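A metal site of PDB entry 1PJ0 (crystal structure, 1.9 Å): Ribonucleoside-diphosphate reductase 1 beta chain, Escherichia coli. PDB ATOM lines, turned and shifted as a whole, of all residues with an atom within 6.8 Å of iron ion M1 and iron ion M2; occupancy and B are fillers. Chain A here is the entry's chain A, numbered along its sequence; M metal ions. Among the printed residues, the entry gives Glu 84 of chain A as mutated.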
ATOM      1  N   GLN A  80     -37.660   6.582 -14.571  1.00  0.00           N
ATOM      2  CA  GLN A  80     -36.221   6.822 -14.673  1.00  0.00           C
ATOM      3  C   GLN A  80     -35.997   8.143 -15.434  1.00  0.00           C
ATOM      4  O   GLN A  80     -35.153   8.973 -15.041  1.00  0.00           O
ATOM      5  CB  GLN A  80     -35.534   5.668 -15.430  1.00  0.00           C
ATOM      6  CG  GLN A  80     -35.715   4.271 -14.794  1.00  0.00           C
ATOM      7  CD  GLN A  80     -35.192   3.135 -15.675  1.00  0.00           C
ATOM      8  OE1 GLN A  80     -35.431   3.107 -16.881  1.00  0.00           O
ATOM      9  NE2 GLN A  80     -34.484   2.179 -15.061  1.00  0.00           N
ATOM     10  N   LEU A  83     -36.672  11.046 -13.042  1.00  0.00           N
ATOM     11  CA  LEU A  83     -35.586  11.236 -12.095  1.00  0.00           C
ATOM     12  C   LEU A  83     -34.346  11.860 -12.733  1.00  0.00           C
ATOM     13  O   LEU A  83     -33.712  12.721 -12.126  1.00  0.00           O
ATOM     14  CB  LEU A  83     -35.202   9.898 -11.454  1.00  0.00           C
ATOM     15  CG  LEU A  83     -36.212   9.203 -10.534  1.00  0.00           C
ATOM     16  CD1 LEU A  83     -35.530   7.991  -9.895  1.00  0.00           C
ATOM     17  CD2 LEU A  83     -36.689  10.152  -9.451  1.00  0.00           C
ATOM     18  N   GLU A  84     -34.007  11.439 -13.952  1.00  0.00           N
ATOM     19  CA  GLU A  84     -32.843  11.975 -14.641  1.00  0.00           C
ATOM     20  C   GLU A  84     -33.046  13.433 -15.012  1.00  0.00           C
ATOM     21  O   GLU A  84     -32.104  14.236 -14.957  1.00  0.00           O
ATOM     22  CB  GLU A  84     -32.527  11.156 -15.909  1.00  0.00           C
ATOM     23  CG  GLU A  84     -32.178   9.699 -15.646  1.00  0.00           C
ATOM     24  CD  GLU A  84     -30.872   9.511 -14.870  1.00  0.00           C
ATOM     25  OE1 GLU A  84     -30.450   8.355 -14.693  1.00  0.00           O
ATOM     26  OE2 GLU A  84     -30.270  10.512 -14.431  1.00  0.00           O
ATOM     27  N   GLN A  87     -32.469  15.273 -11.818  1.00  0.00           N
ATOM     28  CA  GLN A  87     -31.062  15.183 -11.431  1.00  0.00           C
ATOM     29  C   GLN A  87     -30.091  15.848 -12.389  1.00  0.00           C
ATOM     30  O   GLN A  87     -28.948  16.103 -12.034  1.00  0.00           O
ATOM     31  CB  GLN A  87     -30.667  13.722 -11.238  1.00  0.00           C
ATOM     32  CG  GLN A  87     -31.265  13.092  -9.987  1.00  0.00           C
ATOM     33  CD  GLN A  87     -31.026  13.934  -8.747  1.00  0.00           C
ATOM     34  OE1 GLN A  87     -31.808  14.831  -8.428  1.00  0.00           O
ATOM     35  NE2 GLN A  87     -29.938  13.667  -8.049  1.00  0.00           N
ATOM     36  N   TRP A 111     -21.167  15.414 -11.944  1.00  0.00           N
ATOM     37  CA  TRP A 111     -22.236  14.499 -11.566  1.00  0.00           C
ATOM     38  C   TRP A 111     -23.507  14.913 -12.322  1.00  0.00           C
ATOM     39  O   TRP A 111     -24.131  14.091 -13.009  1.00  0.00           O
ATOM     40  CB  TRP A 111     -22.393  14.579 -10.039  1.00  0.00           C
ATOM     41  CG  TRP A 111     -23.682  14.090  -9.438  1.00  0.00           C
ATOM     42  CD1 TRP A 111     -24.571  13.216  -9.986  1.00  0.00           C
ATOM     43  CD2 TRP A 111     -24.176  14.425  -8.139  1.00  0.00           C
ATOM     44  NE1 TRP A 111     -25.605  12.991  -9.100  1.00  0.00           N
ATOM     45  CE2 TRP A 111     -25.383  13.721  -7.956  1.00  0.00           C
ATOM     46  CE3 TRP A 111     -23.726  15.260  -7.108  1.00  0.00           C
ATOM     47  CZ2 TRP A 111     -26.145  13.821  -6.785  1.00  0.00           C
ATOM     48  CZ3 TRP A 111     -24.471  15.360  -5.938  1.00  0.00           C
ATOM     49  CH2 TRP A 111     -25.676  14.641  -5.794  1.00  0.00           C
ATOM     50  N   SER A 114     -23.398  14.144 -16.083  1.00  0.00           N
ATOM     51  CA  SER A 114     -23.584  12.736 -16.421  1.00  0.00           C
ATOM     52  C   SER A 114     -25.071  12.377 -16.370  1.00  0.00           C
ATOM     53  O   SER A 114     -25.515  11.502 -17.105  1.00  0.00           O
ATOM     54  CB  SER A 114     -22.775  11.825 -15.493  1.00  0.00           C
ATOM     55  OG  SER A 114     -23.348  11.743 -14.211  1.00  0.00           O
ATOM     56  N   GLU A 115     -25.838  13.051 -15.520  1.00  0.00           N
ATOM     57  CA  GLU A 115     -27.274  12.756 -15.442  1.00  0.00           C
ATOM     58  C   GLU A 115     -27.956  13.189 -16.743  1.00  0.00           C
ATOM     59  O   GLU A 115     -28.902  12.538 -17.197  1.00  0.00           O
ATOM     60  CB  GLU A 115     -27.923  13.462 -14.231  1.00  0.00           C
ATOM     61  CG  GLU A 115     -27.262  13.148 -12.871  1.00  0.00           C
ATOM     62  CD  GLU A 115     -27.485  11.716 -12.367  1.00  0.00           C
ATOM     63  OE1 GLU A 115     -27.474  10.784 -13.178  1.00  0.00           O
ATOM     64  OE2 GLU A 115     -27.649  11.531 -11.143  1.00  0.00           O
ATOM     65  N   THR A 116     -27.502  14.278 -17.370  1.00  0.00           N
ATOM     66  CA  THR A 116     -28.121  14.693 -18.623  1.00  0.00           C
ATOM     67  C   THR A 116     -27.769  13.702 -19.730  1.00  0.00           C
ATOM     68  O   THR A 116     -28.514  13.563 -20.702  1.00  0.00           O
ATOM     69  CB  THR A 116     -27.712  16.139 -19.078  1.00  0.00           C
ATOM     70  OG1 THR A 116     -26.346  16.152 -19.521  1.00  0.00           O
ATOM     71  CG2 THR A 116     -27.897  17.121 -17.925  1.00  0.00           C
ATOM     72  N   HIS A 118     -27.638  10.580 -19.159  1.00  0.00           N
ATOM     73  CA  HIS A 118     -28.593   9.510 -18.897  1.00  0.00           C
ATOM     74  C   HIS A 118     -29.942   9.898 -19.499  1.00  0.00           C
ATOM     75  O   HIS A 118     -30.668   9.059 -20.042  1.00  0.00           O
ATOM     76  CB  HIS A 118     -28.717   9.286 -17.395  1.00  0.00           C
ATOM     77  CG  HIS A 118     -27.423   8.890 -16.753  1.00  0.00           C
ATOM     78  ND1 HIS A 118     -27.282   8.730 -15.397  1.00  0.00           N
ATOM     79  CD2 HIS A 118     -26.205   8.616 -17.286  1.00  0.00           C
ATOM     80  CE1 HIS A 118     -26.035   8.385 -15.116  1.00  0.00           C
ATOM     81  NE2 HIS A 118     -25.363   8.304 -16.254  1.00  0.00           N
ATOM     82  N   SER A 119     -30.288  11.178 -19.411  1.00  0.00           N
ATOM     83  CA  SER A 119     -31.551  11.654 -19.985  1.00  0.00           C
ATOM     84  C   SER A 119     -31.521  11.459 -21.489  1.00  0.00           C
ATOM     85  O   SER A 119     -32.496  10.994 -22.090  1.00  0.00           O
ATOM     86  CB  SER A 119     -31.749  13.142 -19.675  1.00  0.00           C
ATOM     87  OG  SER A 119     -32.030  13.334 -18.305  1.00  0.00           O
ATOM     88  N   TYR A 122     -32.217   7.922 -22.419  1.00  0.00           N
ATOM     89  CA  TYR A 122     -33.627   7.537 -22.401  1.00  0.00           C
ATOM     90  C   TYR A 122     -34.402   8.070 -23.612  1.00  0.00           C
ATOM     91  O   TYR A 122     -35.363   7.454 -24.051  1.00  0.00           O
ATOM     92  CB  TYR A 122     -34.281   7.957 -21.086  1.00  0.00           C
ATOM     93  CG  TYR A 122     -33.811   7.117 -19.911  1.00  0.00           C
ATOM     94  CD1 TYR A 122     -33.942   5.735 -19.940  1.00  0.00           C
ATOM     95  CD2 TYR A 122     -33.261   7.699 -18.773  1.00  0.00           C
ATOM     96  CE1 TYR A 122     -33.529   4.944 -18.873  1.00  0.00           C
ATOM     97  CE2 TYR A 122     -32.840   6.921 -17.691  1.00  0.00           C
ATOM     98  CZ  TYR A 122     -32.993   5.534 -17.755  1.00  0.00           C
ATOM     99  OH  TYR A 122     -32.599   4.721 -16.705  1.00  0.00           O
ATOM    100  N   GLU A 204     -30.516   8.523  -5.361  1.00  0.00           N
ATOM    101  CA  GLU A 204     -29.423   7.893  -6.092  1.00  0.00           C
ATOM    102  C   GLU A 204     -29.197   6.416  -5.733  1.00  0.00           C
ATOM    103  O   GLU A 204     -28.970   5.583  -6.614  1.00  0.00           O
ATOM    104  CB  GLU A 204     -28.112   8.638  -5.831  1.00  0.00           C
ATOM    105  CG  GLU A 204     -28.051  10.120  -6.232  1.00  0.00           C
ATOM    106  CD  GLU A 204     -27.838  10.338  -7.714  1.00  0.00           C
ATOM    107  OE1 GLU A 204     -27.330   9.424  -8.384  1.00  0.00           O
ATOM    108  OE2 GLU A 204     -28.189  11.433  -8.218  1.00  0.00           O
ATOM    109  N   PHE A 208     -33.176   4.673  -7.978  1.00  0.00           N
ATOM    110  CA  PHE A 208     -32.582   4.278  -9.261  1.00  0.00           C
ATOM    111  C   PHE A 208     -32.331   2.770  -9.328  1.00  0.00           C
ATOM    112  O   PHE A 208     -32.518   2.153 -10.377  1.00  0.00           O
ATOM    113  CB  PHE A 208     -31.236   4.993  -9.506  1.00  0.00           C
ATOM    114  CG  PHE A 208     -31.361   6.362 -10.116  1.00  0.00           C
ATOM    115  CD1 PHE A 208     -32.183   6.595 -11.220  1.00  0.00           C
ATOM    116  CD2 PHE A 208     -30.607   7.440  -9.622  1.00  0.00           C
ATOM    117  CE1 PHE A 208     -32.257   7.849 -11.819  1.00  0.00           C
ATOM    118  CE2 PHE A 208     -30.674   8.697 -10.213  1.00  0.00           C
ATOM    119  CZ  PHE A 208     -31.509   8.898 -11.322  1.00  0.00           C
ATOM    120  N   PHE A 212     -33.609  -0.197 -11.862  1.00  0.00           N
ATOM    121  CA  PHE A 212     -32.667  -1.020 -12.618  1.00  0.00           C
ATOM    122  C   PHE A 212     -33.112  -2.481 -12.579  1.00  0.00           C
ATOM    123  O   PHE A 212     -32.999  -3.205 -13.567  1.00  0.00           O
ATOM    124  CB  PHE A 212     -31.250  -0.924 -12.057  1.00  0.00           C
ATOM    125  CG  PHE A 212     -30.644   0.450 -12.155  1.00  0.00           C
ATOM    126  CD1 PHE A 212     -31.028   1.323 -13.168  1.00  0.00           C
ATOM    127  CD2 PHE A 212     -29.669   0.857 -11.248  1.00  0.00           C
ATOM    128  CE1 PHE A 212     -30.453   2.590 -13.266  1.00  0.00           C
ATOM    129  CE2 PHE A 212     -29.087   2.113 -11.334  1.00  0.00           C
ATOM    130  CZ  PHE A 212     -29.477   2.983 -12.354  1.00  0.00           C
ATOM    131  N   ILE A 234     -25.469   3.347 -17.132  1.00  0.00           N
ATOM    132  CA  ILE A 234     -26.061   4.307 -16.216  1.00  0.00           C
ATOM    133  C   ILE A 234     -25.800   3.902 -14.775  1.00  0.00           C
ATOM    134  O   ILE A 234     -25.395   4.732 -13.957  1.00  0.00           O
ATOM    135  CB  ILE A 234     -27.598   4.422 -16.448  1.00  0.00           C
ATOM    136  CG1 ILE A 234     -27.861   5.184 -17.743  1.00  0.00           C
ATOM    137  CG2 ILE A 234     -28.276   5.123 -15.249  1.00  0.00           C
ATOM    138  CD1 ILE A 234     -29.344   5.335 -18.083  1.00  0.00           C
ATOM    139  N   ASP A 237     -22.520   4.757 -13.365  1.00  0.00           N
ATOM    140  CA  ASP A 237     -22.447   6.155 -12.945  1.00  0.00           C
ATOM    141  C   ASP A 237     -23.142   6.396 -11.605  1.00  0.00           C
ATOM    142  O   ASP A 237     -22.584   7.059 -10.736  1.00  0.00           O
ATOM    143  CB  ASP A 237     -23.094   7.080 -13.988  1.00  0.00           C
ATOM    144  CG  ASP A 237     -22.299   7.174 -15.268  1.00  0.00           C
ATOM    145  OD1 ASP A 237     -21.112   6.771 -15.279  1.00  0.00           O
ATOM    146  OD2 ASP A 237     -22.863   7.654 -16.270  1.00  0.00           O
ATOM    147  N   GLU A 238     -24.342   5.859 -11.439  1.00  0.00           N
ATOM    148  CA  GLU A 238     -25.077   6.033 -10.193  1.00  0.00           C
ATOM    149  C   GLU A 238     -24.268   5.512  -8.991  1.00  0.00           C
ATOM    150  O   GLU A 238     -24.390   6.031  -7.884  1.00  0.00           O
ATOM    151  CB  GLU A 238     -26.446   5.333 -10.231  1.00  0.00           C
ATOM    152  CG  GLU A 238     -27.382   5.788 -11.360  1.00  0.00           C
ATOM    153  CD  GLU A 238     -27.549   7.299 -11.431  1.00  0.00           C
ATOM    154  OE1 GLU A 238     -27.239   8.001 -10.445  1.00  0.00           O
ATOM    155  OE2 GLU A 238     -27.996   7.798 -12.492  1.00  0.00           O
ATOM    156  N   ALA A 239     -23.445   4.488  -9.227  1.00  0.00           N
ATOM    157  CA  ALA A 239     -22.614   3.936  -8.148  1.00  0.00           C
ATOM    158  C   ALA A 239     -21.619   5.010  -7.679  1.00  0.00           C
ATOM    159  O   ALA A 239     -21.327   5.111  -6.481  1.00  0.00           O
ATOM    160  CB  ALA A 239     -21.869   2.702  -8.657  1.00  0.00           C
ATOM    161  N   HIS A 241     -22.123   8.292  -8.063  1.00  0.00           N
ATOM    162  CA  HIS A 241     -22.946   9.350  -7.497  1.00  0.00           C
ATOM    163  C   HIS A 241     -23.319   9.105  -6.039  1.00  0.00           C
ATOM    164  O   HIS A 241     -23.213  10.001  -5.209  1.00  0.00           O
ATOM    165  CB  HIS A 241     -24.206   9.532  -8.329  1.00  0.00           C
ATOM    166  CG  HIS A 241     -23.927   9.892  -9.759  1.00  0.00           C
ATOM    167  ND1 HIS A 241     -24.922   9.974 -10.713  1.00  0.00           N
ATOM    168  CD2 HIS A 241     -22.768  10.181 -10.401  1.00  0.00           C
ATOM    169  CE1 HIS A 241     -24.373  10.294 -11.880  1.00  0.00           C
ATOM    170  NE2 HIS A 241     -23.071  10.429 -11.713  1.00  0.00           N
ATOM    171  N   LEU A 242     -23.743   7.887  -5.717  1.00  0.00           N
ATOM    172  CA  LEU A 242     -24.107   7.605  -4.338  1.00  0.00           C
ATOM    173  C   LEU A 242     -22.851   7.466  -3.491  1.00  0.00           C
ATOM    174  O   LEU A 242     -22.880   7.653  -2.269  1.00  0.00           O
ATOM    175  CB  LEU A 242     -24.992   6.344  -4.265  1.00  0.00           C
ATOM    176  CG  LEU A 242     -24.398   4.976  -4.580  1.00  0.00           C
ATOM    177  CD1 LEU A 242     -23.701   4.431  -3.335  1.00  0.00           C
ATOM    178  CD2 LEU A 242     -25.519   4.013  -4.989  1.00  0.00           C
HETATM  179 FE    FE M   1     -26.982   9.906 -10.298  1.00  0.00          FE
HETATM  180 FE    FE M   2     -28.624   9.094 -13.814  1.00  0.00          FE
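CZ of Phe 208 touches iron ion M2, at 3.8 Å.
Iron ion M2 is bound by the side-chain carboxylate (OE2) of Glu 238 (2.0 Å), a ring nitrogen (ND1) of His 118 (2.1 Å), the side-chain carboxylate (OE1) of Glu 115 (2.1 Å), the side-chain carboxylate (OE1) of Glu 84 (2.2 Å) and the side-chain carboxylate (OE2) of Glu 84 (2.3 Å).
The side-chain hydroxyl (OG) of Ser 114 sits at hydrogen-bond distance from a ring nitrogen (NE2) of His 241, 2.8 Å away. OG of Ser 119 sits close to O of Glu 84 (3.5 Å). The side-chain carboxylate of Glu 204 lies within hydrogen-bond range of the indole nitrogen of Trp 111 (3.1 Å). The backbone carbonyl oxygen (O) of Trp 111 is in hydrogen-bond range of the side-chain hydroxyl (OG) of Ser 114, at 2.8 Å. NE2 of Gln 87 sits at hydrogen-bond distance from OE2 of Glu 204, 2.8 Å away. The backbone carbonyl oxygen (O) of Ser 114 lies close to a ring nitrogen (NE2) of His 118, at 3.3 Å. O of Glu 115 sits at hydrogen-bond distance from OG of Ser 119, 3.4 Å away. A ring nitrogen (ND1) of His 241 sits close to the indole nitrogen (NE1) of Trp 111 (3.5 Å).
Iron ion M1 is bound by OE1 of Glu 238 (1.9 Å), OE2 of Glu 115 (1.9 Å), OE1 of Glu 204 (2.0 Å) and ND1 of His 241 (2.1 Å). Iron ion M1 has four donor atoms within binding distance. Slightly farther from iron ion M1 lies OE2 of Glu 204 (2.8 Å).
NE1 of Trp 111 touches iron ion M1, 3.6 Å away. CE2 of Phe 208 touches iron ion M1, 3.9 Å away. Of the 20 residues printed, 6 come within 4 Å of iron ion M1. The nearest printed residue that does not touch iron ion M1 is His 118 (5.1 Å).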
